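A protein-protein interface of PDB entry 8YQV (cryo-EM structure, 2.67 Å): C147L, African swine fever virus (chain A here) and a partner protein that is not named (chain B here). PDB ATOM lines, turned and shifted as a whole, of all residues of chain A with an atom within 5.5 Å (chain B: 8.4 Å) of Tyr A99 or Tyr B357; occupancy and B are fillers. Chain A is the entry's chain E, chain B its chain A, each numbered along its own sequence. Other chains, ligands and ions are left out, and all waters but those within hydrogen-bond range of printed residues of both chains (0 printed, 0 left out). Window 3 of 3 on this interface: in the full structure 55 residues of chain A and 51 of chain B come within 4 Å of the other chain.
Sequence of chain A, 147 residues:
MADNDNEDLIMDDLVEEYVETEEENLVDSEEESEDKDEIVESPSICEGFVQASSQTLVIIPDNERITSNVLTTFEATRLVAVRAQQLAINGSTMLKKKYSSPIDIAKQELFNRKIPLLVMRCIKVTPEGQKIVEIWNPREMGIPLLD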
ATOM      1  N   ALA A  84      17.491 -22.307 -27.775  1.00  0.00           N
ATOM      2  CA  ALA A  84      16.148 -21.744 -27.794  1.00  0.00           C
ATOM      3  C   ALA A  84      15.971 -20.761 -28.942  1.00  0.00           C
ATOM      4  O   ALA A  84      14.935 -20.768 -29.612  1.00  0.00           O
ATOM      5  CB  ALA A  84      15.850 -21.071 -26.459  1.00  0.00           C
ATOM      6  N   LEU A  87      15.739 -22.710 -32.102  1.00  0.00           N
ATOM      7  CA  LEU A  87      14.414 -23.305 -32.219  1.00  0.00           C
ATOM      8  C   LEU A  87      13.372 -22.272 -32.607  1.00  0.00           C
ATOM      9  O   LEU A  87      12.404 -22.601 -33.297  1.00  0.00           O
ATOM     10  CB  LEU A  87      14.009 -23.973 -30.908  1.00  0.00           C
ATOM     11  CG  LEU A  87      14.627 -25.341 -30.665  1.00  0.00           C
ATOM     12  CD1 LEU A  87      14.651 -25.640 -29.193  1.00  0.00           C
ATOM     13  CD2 LEU A  87      13.853 -26.396 -31.413  1.00  0.00           C
ATOM     14  N   ALA A  88      13.542 -21.032 -32.159  1.00  0.00           N
ATOM     15  CA  ALA A  88      12.715 -19.949 -32.667  1.00  0.00           C
ATOM     16  C   ALA A  88      12.928 -19.733 -34.156  1.00  0.00           C
ATOM     17  O   ALA A  88      12.040 -19.200 -34.824  1.00  0.00           O
ATOM     18  CB  ALA A  88      12.994 -18.658 -31.905  1.00  0.00           C
ATOM     19  N   GLY A  91      12.682 -24.806 -35.365  1.00  0.00           N
ATOM     20  CA  GLY A  91      11.672 -25.619 -34.728  1.00  0.00           C
ATOM     21  C   GLY A  91      11.861 -27.112 -34.875  1.00  0.00           C
ATOM     22  O   GLY A  91      11.033 -27.873 -34.365  1.00  0.00           O
ATOM     23  N   LEU A  95      13.407 -33.982 -29.523  1.00  0.00           N
ATOM     24  CA  LEU A  95      12.734 -34.184 -28.250  1.00  0.00           C
ATOM     25  C   LEU A  95      11.397 -34.881 -28.477  1.00  0.00           C
ATOM     26  O   LEU A  95      10.606 -34.467 -29.329  1.00  0.00           O
ATOM     27  CB  LEU A  95      12.536 -32.836 -27.563  1.00  0.00           C
ATOM     28  CG  LEU A  95      12.267 -32.774 -26.066  1.00  0.00           C
ATOM     29  CD1 LEU A  95      13.524 -33.091 -25.298  1.00  0.00           C
ATOM     30  CD2 LEU A  95      11.754 -31.399 -25.706  1.00  0.00           C
ATOM     31  N   LYS A  97       8.697 -35.326 -26.415  1.00  0.00           N
ATOM     32  CA  LYS A  97       7.505 -34.678 -25.896  1.00  0.00           C
ATOM     33  C   LYS A  97       7.332 -33.304 -26.526  1.00  0.00           C
ATOM     34  O   LYS A  97       8.301 -32.661 -26.933  1.00  0.00           O
ATOM     35  CB  LYS A  97       7.565 -34.548 -24.374  1.00  0.00           C
ATOM     36  CG  LYS A  97       6.200 -34.577 -23.724  1.00  0.00           C
ATOM     37  CD  LYS A  97       6.273 -34.635 -22.214  1.00  0.00           C
ATOM     38  CE  LYS A  97       6.170 -33.246 -21.615  1.00  0.00           C
ATOM     39  NZ  LYS A  97       5.953 -33.285 -20.144  1.00  0.00           N
ATOM     40  N   LYS A  98       6.083 -32.858 -26.601  1.00  0.00           N
ATOM     41  CA  LYS A  98       5.752 -31.602 -27.257  1.00  0.00           C
ATOM     42  C   LYS A  98       5.627 -30.474 -26.244  1.00  0.00           C
ATOM     43  O   LYS A  98       4.985 -30.625 -25.201  1.00  0.00           O
ATOM     44  CB  LYS A  98       4.453 -31.738 -28.047  1.00  0.00           C
ATOM     45  CG  LYS A  98       4.358 -33.018 -28.847  1.00  0.00           C
ATOM     46  CD  LYS A  98       5.385 -33.047 -29.962  1.00  0.00           C
ATOM     47  CE  LYS A  98       5.268 -31.826 -30.856  1.00  0.00           C
ATOM     48  NZ  LYS A  98       6.040 -31.989 -32.118  1.00  0.00           N
ATOM     49  N   TYR A  99       6.241 -29.340 -26.566  1.00  0.00           N
ATOM     50  CA  TYR A  99       6.195 -28.139 -25.751  1.00  0.00           C
ATOM     51  C   TYR A  99       5.810 -26.970 -26.642  1.00  0.00           C
ATOM     52  O   TYR A  99       5.944 -27.026 -27.864  1.00  0.00           O
ATOM     53  CB  TYR A  99       7.540 -27.876 -25.062  1.00  0.00           C
ATOM     54  CG  TYR A  99       7.910 -28.910 -24.026  1.00  0.00           C
ATOM     55  CD1 TYR A  99       7.578 -28.735 -22.693  1.00  0.00           C
ATOM     56  CD2 TYR A  99       8.583 -30.064 -24.386  1.00  0.00           C
ATOM     57  CE1 TYR A  99       7.914 -29.680 -21.748  1.00  0.00           C
ATOM     58  CE2 TYR A  99       8.919 -31.010 -23.453  1.00  0.00           C
ATOM     59  CZ  TYR A  99       8.580 -30.815 -22.136  1.00  0.00           C
ATOM     60  OH  TYR A  99       8.917 -31.765 -21.203  1.00  0.00           O
ATOM     61  N   SER A 100       5.315 -25.901 -26.024  1.00  0.00           N
ATOM     62  CA  SER A 100       4.822 -24.745 -26.761  1.00  0.00           C
ATOM     63  C   SER A 100       5.761 -23.549 -26.677  1.00  0.00           C
ATOM     64  O   SER A 100       5.381 -22.440 -27.059  1.00  0.00           O
ATOM     65  CB  SER A 100       3.432 -24.359 -26.265  1.00  0.00           C
ATOM     66  OG  SER A 100       3.176 -22.995 -26.522  1.00  0.00           O
ATOM     67  N   SER A 101       6.976 -23.747 -26.182  1.00  0.00           N
ATOM     68  CA  SER A 101       7.946 -22.676 -26.041  1.00  0.00           C
ATOM     69  C   SER A 101       9.300 -23.174 -26.516  1.00  0.00           C
ATOM     70  O   SER A 101       9.618 -24.356 -26.350  1.00  0.00           O
ATOM     71  CB  SER A 101       8.049 -22.207 -24.583  1.00  0.00           C
ATOM     72  OG  SER A 101       8.937 -21.116 -24.453  1.00  0.00           O
ATOM     73  N   PRO A 102      10.108 -22.308 -27.131  1.00  0.00           N
ATOM     74  CA  PRO A 102      11.485 -22.708 -27.443  1.00  0.00           C
ATOM     75  C   PRO A 102      12.314 -22.955 -26.203  1.00  0.00           C
ATOM     76  O   PRO A 102      13.197 -23.817 -26.219  1.00  0.00           O
ATOM     77  CB  PRO A 102      12.027 -21.516 -28.242  1.00  0.00           C
ATOM     78  CG  PRO A 102      10.852 -20.691 -28.578  1.00  0.00           C
ATOM     79  CD  PRO A 102       9.853 -20.914 -27.509  1.00  0.00           C
ATOM     80  N   ASP A 104      11.385 -24.090 -23.158  1.00  0.00           N
ATOM     81  CA  ASP A 104      11.103 -25.390 -22.564  1.00  0.00           C
ATOM     82  C   ASP A 104      11.700 -26.519 -23.391  1.00  0.00           C
ATOM     83  O   ASP A 104      12.267 -27.468 -22.837  1.00  0.00           O
ATOM     84  CB  ASP A 104       9.601 -25.577 -22.405  1.00  0.00           C
ATOM     85  CG  ASP A 104       9.086 -25.017 -21.100  1.00  0.00           C
ATOM     86  OD1 ASP A 104       9.917 -24.677 -20.234  1.00  0.00           O
ATOM     87  OD2 ASP A 104       7.851 -24.914 -20.941  1.00  0.00           O
ATOM     88  N   ILE A 105      11.597 -26.428 -24.717  1.00  0.00           N
ATOM     89  CA  ILE A 105      12.199 -27.441 -25.578  1.00  0.00           C
ATOM     90  C   ILE A 105      13.705 -27.486 -25.378  1.00  0.00           C
ATOM     91  O   ILE A 105      14.294 -28.564 -25.271  1.00  0.00           O
ATOM     92  CB  ILE A 105      11.840 -27.181 -27.052  1.00  0.00           C
ATOM     93  CG1 ILE A 105      10.334 -27.229 -27.262  1.00  0.00           C
ATOM     94  CG2 ILE A 105      12.494 -28.207 -27.937  1.00  0.00           C
ATOM     95  CD1 ILE A 105       9.904 -26.744 -28.618  1.00  0.00           C
ATOM     96  N   GLN A 108      14.613 -29.038 -21.945  1.00  0.00           N
ATOM     97  CA  GLN A 108      14.456 -30.485 -21.926  1.00  0.00           C
ATOM     98  C   GLN A 108      15.460 -31.179 -22.830  1.00  0.00           C
ATOM     99  O   GLN A 108      15.845 -32.315 -22.550  1.00  0.00           O
ATOM    100  CB  GLN A 108      13.040 -30.874 -22.334  1.00  0.00           C
ATOM    101  CG  GLN A 108      11.972 -30.263 -21.471  1.00  0.00           C
ATOM    102  CD  GLN A 108      12.117 -30.621 -20.015  1.00  0.00           C
ATOM    103  OE1 GLN A 108      12.443 -31.754 -19.671  1.00  0.00           O
ATOM    104  NE2 GLN A 108      11.877 -29.649 -19.146  1.00  0.00           N
ATOM    105  N   GLU B 352       7.460 -12.965 -29.575  1.00  0.00           N
ATOM    106  CA  GLU B 352       7.234 -14.394 -29.771  1.00  0.00           C
ATOM    107  C   GLU B 352       7.312 -14.696 -31.262  1.00  0.00           C
ATOM    108  O   GLU B 352       6.473 -14.228 -32.034  1.00  0.00           O
ATOM    109  CB  GLU B 352       5.876 -14.814 -29.218  1.00  0.00           C
ATOM    110  CG  GLU B 352       5.672 -14.580 -27.740  1.00  0.00           C
ATOM    111  CD  GLU B 352       6.155 -15.729 -26.891  1.00  0.00           C
ATOM    112  OE1 GLU B 352       6.224 -16.858 -27.406  1.00  0.00           O
ATOM    113  OE2 GLU B 352       6.443 -15.508 -25.700  1.00  0.00           O
ATOM    114  N   THR B 353       8.303 -15.479 -31.667  1.00  0.00           N
ATOM    115  CA  THR B 353       8.402 -15.906 -33.056  1.00  0.00           C
ATOM    116  C   THR B 353       7.403 -17.025 -33.302  1.00  0.00           C
ATOM    117  O   THR B 353       7.405 -18.030 -32.589  1.00  0.00           O
ATOM    118  CB  THR B 353       9.819 -16.368 -33.382  1.00  0.00           C
ATOM    119  OG1 THR B 353      10.746 -15.331 -33.049  1.00  0.00           O
ATOM    120  CG2 THR B 353       9.945 -16.681 -34.852  1.00  0.00           C
ATOM    121  N   VAL B 354       6.549 -16.853 -34.308  1.00  0.00           N
ATOM    122  CA  VAL B 354       5.488 -17.817 -34.566  1.00  0.00           C
ATOM    123  C   VAL B 354       6.093 -19.061 -35.201  1.00  0.00           C
ATOM    124  O   VAL B 354       6.780 -18.983 -36.225  1.00  0.00           O
ATOM    125  CB  VAL B 354       4.401 -17.212 -35.463  1.00  0.00           C
ATOM    126  CG1 VAL B 354       3.334 -18.245 -35.762  1.00  0.00           C
ATOM    127  CG2 VAL B 354       3.800 -15.980 -34.817  1.00  0.00           C
ATOM    128  N   GLN B 355       5.843 -20.214 -34.594  1.00  0.00           N
ATOM    129  CA  GLN B 355       6.284 -21.496 -35.112  1.00  0.00           C
ATOM    130  C   GLN B 355       5.136 -22.487 -34.983  1.00  0.00           C
ATOM    131  O   GLN B 355       4.065 -22.162 -34.471  1.00  0.00           O
ATOM    132  CB  GLN B 355       7.532 -21.996 -34.378  1.00  0.00           C
ATOM    133  CG  GLN B 355       8.810 -21.243 -34.697  1.00  0.00           C
ATOM    134  CD  GLN B 355       9.256 -21.422 -36.130  1.00  0.00           C
ATOM    135  OE1 GLN B 355       9.340 -20.462 -36.889  1.00  0.00           O
ATOM    136  NE2 GLN B 355       9.542 -22.660 -36.509  1.00  0.00           N
ATOM    137  N   HIS B 356       5.359 -23.712 -35.452  1.00  0.00           N
ATOM    138  CA  HIS B 356       4.290 -24.701 -35.429  1.00  0.00           C
ATOM    139  C   HIS B 356       3.921 -25.123 -34.016  1.00  0.00           C
ATOM    140  O   HIS B 356       2.803 -25.599 -33.801  1.00  0.00           O
ATOM    141  CB  HIS B 356       4.682 -25.929 -36.247  1.00  0.00           C
ATOM    142  CG  HIS B 356       5.909 -26.626 -35.745  1.00  0.00           C
ATOM    143  ND1 HIS B 356       7.177 -26.299 -36.172  1.00  0.00           N
ATOM    144  CD2 HIS B 356       6.059 -27.641 -34.862  1.00  0.00           C
ATOM    145  CE1 HIS B 356       8.057 -27.077 -35.569  1.00  0.00           C
ATOM    146  NE2 HIS B 356       7.405 -27.900 -34.767  1.00  0.00           N
ATOM    147  N   TYR B 357       4.823 -24.960 -33.052  1.00  0.00           N
ATOM    148  CA  TYR B 357       4.571 -25.427 -31.696  1.00  0.00           C
ATOM    149  C   TYR B 357       3.868 -24.399 -30.821  1.00  0.00           C
ATOM    150  O   TYR B 357       3.419 -24.753 -29.728  1.00  0.00           O
ATOM    151  CB  TYR B 357       5.882 -25.855 -31.024  1.00  0.00           C
ATOM    152  CG  TYR B 357       7.006 -24.854 -31.137  1.00  0.00           C
ATOM    153  CD1 TYR B 357       7.009 -23.702 -30.372  1.00  0.00           C
ATOM    154  CD2 TYR B 357       8.069 -25.069 -31.989  1.00  0.00           C
ATOM    155  CE1 TYR B 357       8.020 -22.792 -30.467  1.00  0.00           C
ATOM    156  CE2 TYR B 357       9.090 -24.161 -32.086  1.00  0.00           C
ATOM    157  CZ  TYR B 357       9.058 -23.025 -31.320  1.00  0.00           C
ATOM    158  OH  TYR B 357      10.071 -22.106 -31.409  1.00  0.00           O
ATOM    159  N   ASN B 358       3.744 -23.146 -31.266  1.00  0.00           N
ATOM    160  CA  ASN B 358       3.096 -22.124 -30.453  1.00  0.00           C
ATOM    161  C   ASN B 358       2.065 -21.320 -31.236  1.00  0.00           C
ATOM    162  O   ASN B 358       1.671 -20.241 -30.792  1.00  0.00           O
ATOM    163  CB  ASN B 358       4.126 -21.173 -29.841  1.00  0.00           C
ATOM    164  CG  ASN B 358       4.949 -20.458 -30.883  1.00  0.00           C
ATOM    165  OD1 ASN B 358       4.836 -20.729 -32.071  1.00  0.00           O
ATOM    166  ND2 ASN B 358       5.777 -19.526 -30.441  1.00  0.00           N
ATOM    167  N   ILE B 359       1.624 -21.809 -32.392  1.00  0.00           N
ATOM    168  CA  ILE B 359       0.653 -21.053 -33.172  1.00  0.00           C
ATOM    169  C   ILE B 359      -0.694 -21.024 -32.462  1.00  0.00           C
ATOM    170  O   ILE B 359      -1.398 -20.008 -32.479  1.00  0.00           O
ATOM    171  CB  ILE B 359       0.545 -21.621 -34.599  1.00  0.00           C
ATOM    172  CG1 ILE B 359      -0.510 -20.861 -35.394  1.00  0.00           C
ATOM    173  CG2 ILE B 359       0.234 -23.104 -34.572  1.00  0.00           C
ATOM    174  CD1 ILE B 359      -0.214 -19.395 -35.540  1.00  0.00           C
ATOM    175  N   ASN B 360      -1.072 -22.128 -31.814  1.00  0.00           N
ATOM    176  CA  ASN B 360      -2.345 -22.162 -31.105  1.00  0.00           C
ATOM    177  C   ASN B 360      -2.304 -21.334 -29.831  1.00  0.00           C
ATOM    178  O   ASN B 360      -3.305 -20.708 -29.470  1.00  0.00           O
ATOM    179  CB  ASN B 360      -2.727 -23.604 -30.784  1.00  0.00           C
ATOM    180  CG  ASN B 360      -3.072 -24.397 -32.020  1.00  0.00           C
ATOM    181  OD1 ASN B 360      -3.750 -23.901 -32.918  1.00  0.00           O
ATOM    182  ND2 ASN B 360      -2.607 -25.638 -32.075  1.00  0.00           N
ATOM    183  N   ARG B 361      -1.168 -21.317 -29.138  1.00  0.00           N
ATOM    184  CA  ARG B 361      -1.064 -20.553 -27.902  1.00  0.00           C
ATOM    185  C   ARG B 361      -1.064 -19.054 -28.163  1.00  0.00           C
ATOM    186  O   ARG B 361      -1.594 -18.284 -27.358  1.00  0.00           O
ATOM    187  CB  ARG B 361       0.196 -20.958 -27.141  1.00  0.00           C
ATOM    188  CG  ARG B 361       0.411 -20.185 -25.861  1.00  0.00           C
ATOM    189  CD  ARG B 361       1.599 -20.707 -25.095  1.00  0.00           C
ATOM    190  NE  ARG B 361       2.828 -20.621 -25.871  1.00  0.00           N
ATOM    191  CZ  ARG B 361       3.583 -19.537 -25.958  1.00  0.00           C
ATOM    192  NH1 ARG B 361       3.258 -18.419 -25.333  1.00  0.00           N
ATOM    193  NH2 ARG B 361       4.693 -19.576 -26.687  1.00  0.00           N
ATOM    194  N   LEU B 362      -0.474 -18.622 -29.275  1.00  0.00           N
ATOM    195  CA  LEU B 362      -0.367 -17.201 -29.569  1.00  0.00           C
ATOM    196  C   LEU B 362      -1.607 -16.626 -30.232  1.00  0.00           C
ATOM    197  O   LEU B 362      -1.729 -15.401 -30.310  1.00  0.00           O
ATOM    198  CB  LEU B 362       0.844 -16.936 -30.459  1.00  0.00           C
ATOM    199  CG  LEU B 362       2.206 -17.193 -29.827  1.00  0.00           C
ATOM    200  CD1 LEU B 362       3.300 -16.772 -30.779  1.00  0.00           C
ATOM    201  CD2 LEU B 362       2.321 -16.467 -28.508  1.00  0.00           C
ATOM    202  N   VAL B 401       4.175 -18.797 -40.075  1.00  0.00           N
ATOM    203  CA  VAL B 401       5.344 -19.332 -39.390  1.00  0.00           C
ATOM    204  C   VAL B 401       6.547 -18.469 -39.738  1.00  0.00           C
ATOM    205  O   VAL B 401       6.934 -18.359 -40.905  1.00  0.00           O
ATOM    206  CB  VAL B 401       5.582 -20.797 -39.769  1.00  0.00           C
ATOM    207  CG1 VAL B 401       6.984 -21.210 -39.398  1.00  0.00           C
ATOM    208  CG2 VAL B 401       4.575 -21.682 -39.073  1.00  0.00           C
ATOM    209  N   VAL B 471      14.641 -14.072 -26.685  1.00  0.00           N
ATOM    210  CA  VAL B 471      14.678 -15.437 -26.173  1.00  0.00           C
ATOM    211  C   VAL B 471      15.950 -15.693 -25.375  1.00  0.00           C
ATOM    212  O   VAL B 471      15.907 -16.312 -24.309  1.00  0.00           O
ATOM    213  CB  VAL B 471      14.527 -16.444 -27.324  1.00  0.00           C
ATOM    214  CG1 VAL B 471      14.450 -17.830 -26.786  1.00  0.00           C
ATOM    215  CG2 VAL B 471      13.290 -16.148 -28.112  1.00  0.00           C
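CG1 of Val B471 touches CB of Ala A84, at 3.5 Å. Thr B353 touches Ala A88 (CG2 to O, 3.3 Å). Gln B355 touches Ala A88 (OE1 to O, 3.6 Å). NE2 of Gln B355 touches N of Gly A91, 3.97 Å away. Gly A91 touches His B356 (O to CE1, 3.3 Å). CA of Gly A91 touches CE2 of Tyr B357 (3.97 Å). Tyr A99 touches Tyr B357. Ser A100 touches Tyr B357. CB of Asn B358 touches O of Ser A100, 3.3 Å away. CG of Pro A102 touches OH of Tyr B357 (3.3 Å).
The side-chain hydroxyl (OH) of Tyr B357 lies within hydrogen-bond range of the backbone carbonyl oxygen (O) of Leu A87 (3.0 Å). OG of Ser A100 sits at hydrogen-bond distance from NE of Arg B361 (2.5 Å).
Printed residues of chain A that touch a printed residue of chain B: Ala A84, Leu A87, Ala A88, Gly A91, Tyr A99, Ser A100 and Pro A102. Along chain A the printed residues that touch a printed residue of chain B span positions 84 to 102. Among the printed residues, 13 pairs touch across the chains.
NH2 of Arg B361 lies within salt-bridge range of OE1 of Glu B352 (3.2 Å). O of Thr B353 lies within hydrogen-bond range of ND2 of Asn B358. The side-chain amide oxygen of Asn B358 sits at hydrogen-bond distance from the backbone NH of Gln B355. The side-chain amino group (NZ) of Lys A97 sits close to the side-chain hydroxyl (OH) of Tyr A99 (3.5 Å).
Tyr A99 touches just one residue of chain B: Tyr B357. Of the printed residues of chain A, Tyr B357 touches Leu A87, Ala A88, Gly A91, Tyr A99, Ser A100 and Pro A102. Of chain B, only Tyr B357, Asn B358 and Arg B361 come within 4 Å of Ser A100. Of the printed residues of chain A, Val B471 touches Ala A84 (3.5 Å). Of the printed residues of chain A, Arg B361 touches Ser A100 (2.5 Å). Of the printed residues of chain A, Gln B355 touches Ala A88 (3.6 Å) and Gly A91 (3.97 Å). Of the printed residues of chain A, Thr B353 touches Ala A88 (3.3 Å). Printed residues of chain B within 4 Å of Gly A91: Gln B355 (3.97 Å), His B356 (3.3 Å) and Tyr B357 (3.97 Å). The nearest printed residue of chain A that does not touch Tyr B357 is Ser A101 (4.2 Å). The nearest printed residue of chain A that does not touch Val B471 is Ala A88 (4.6 Å).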
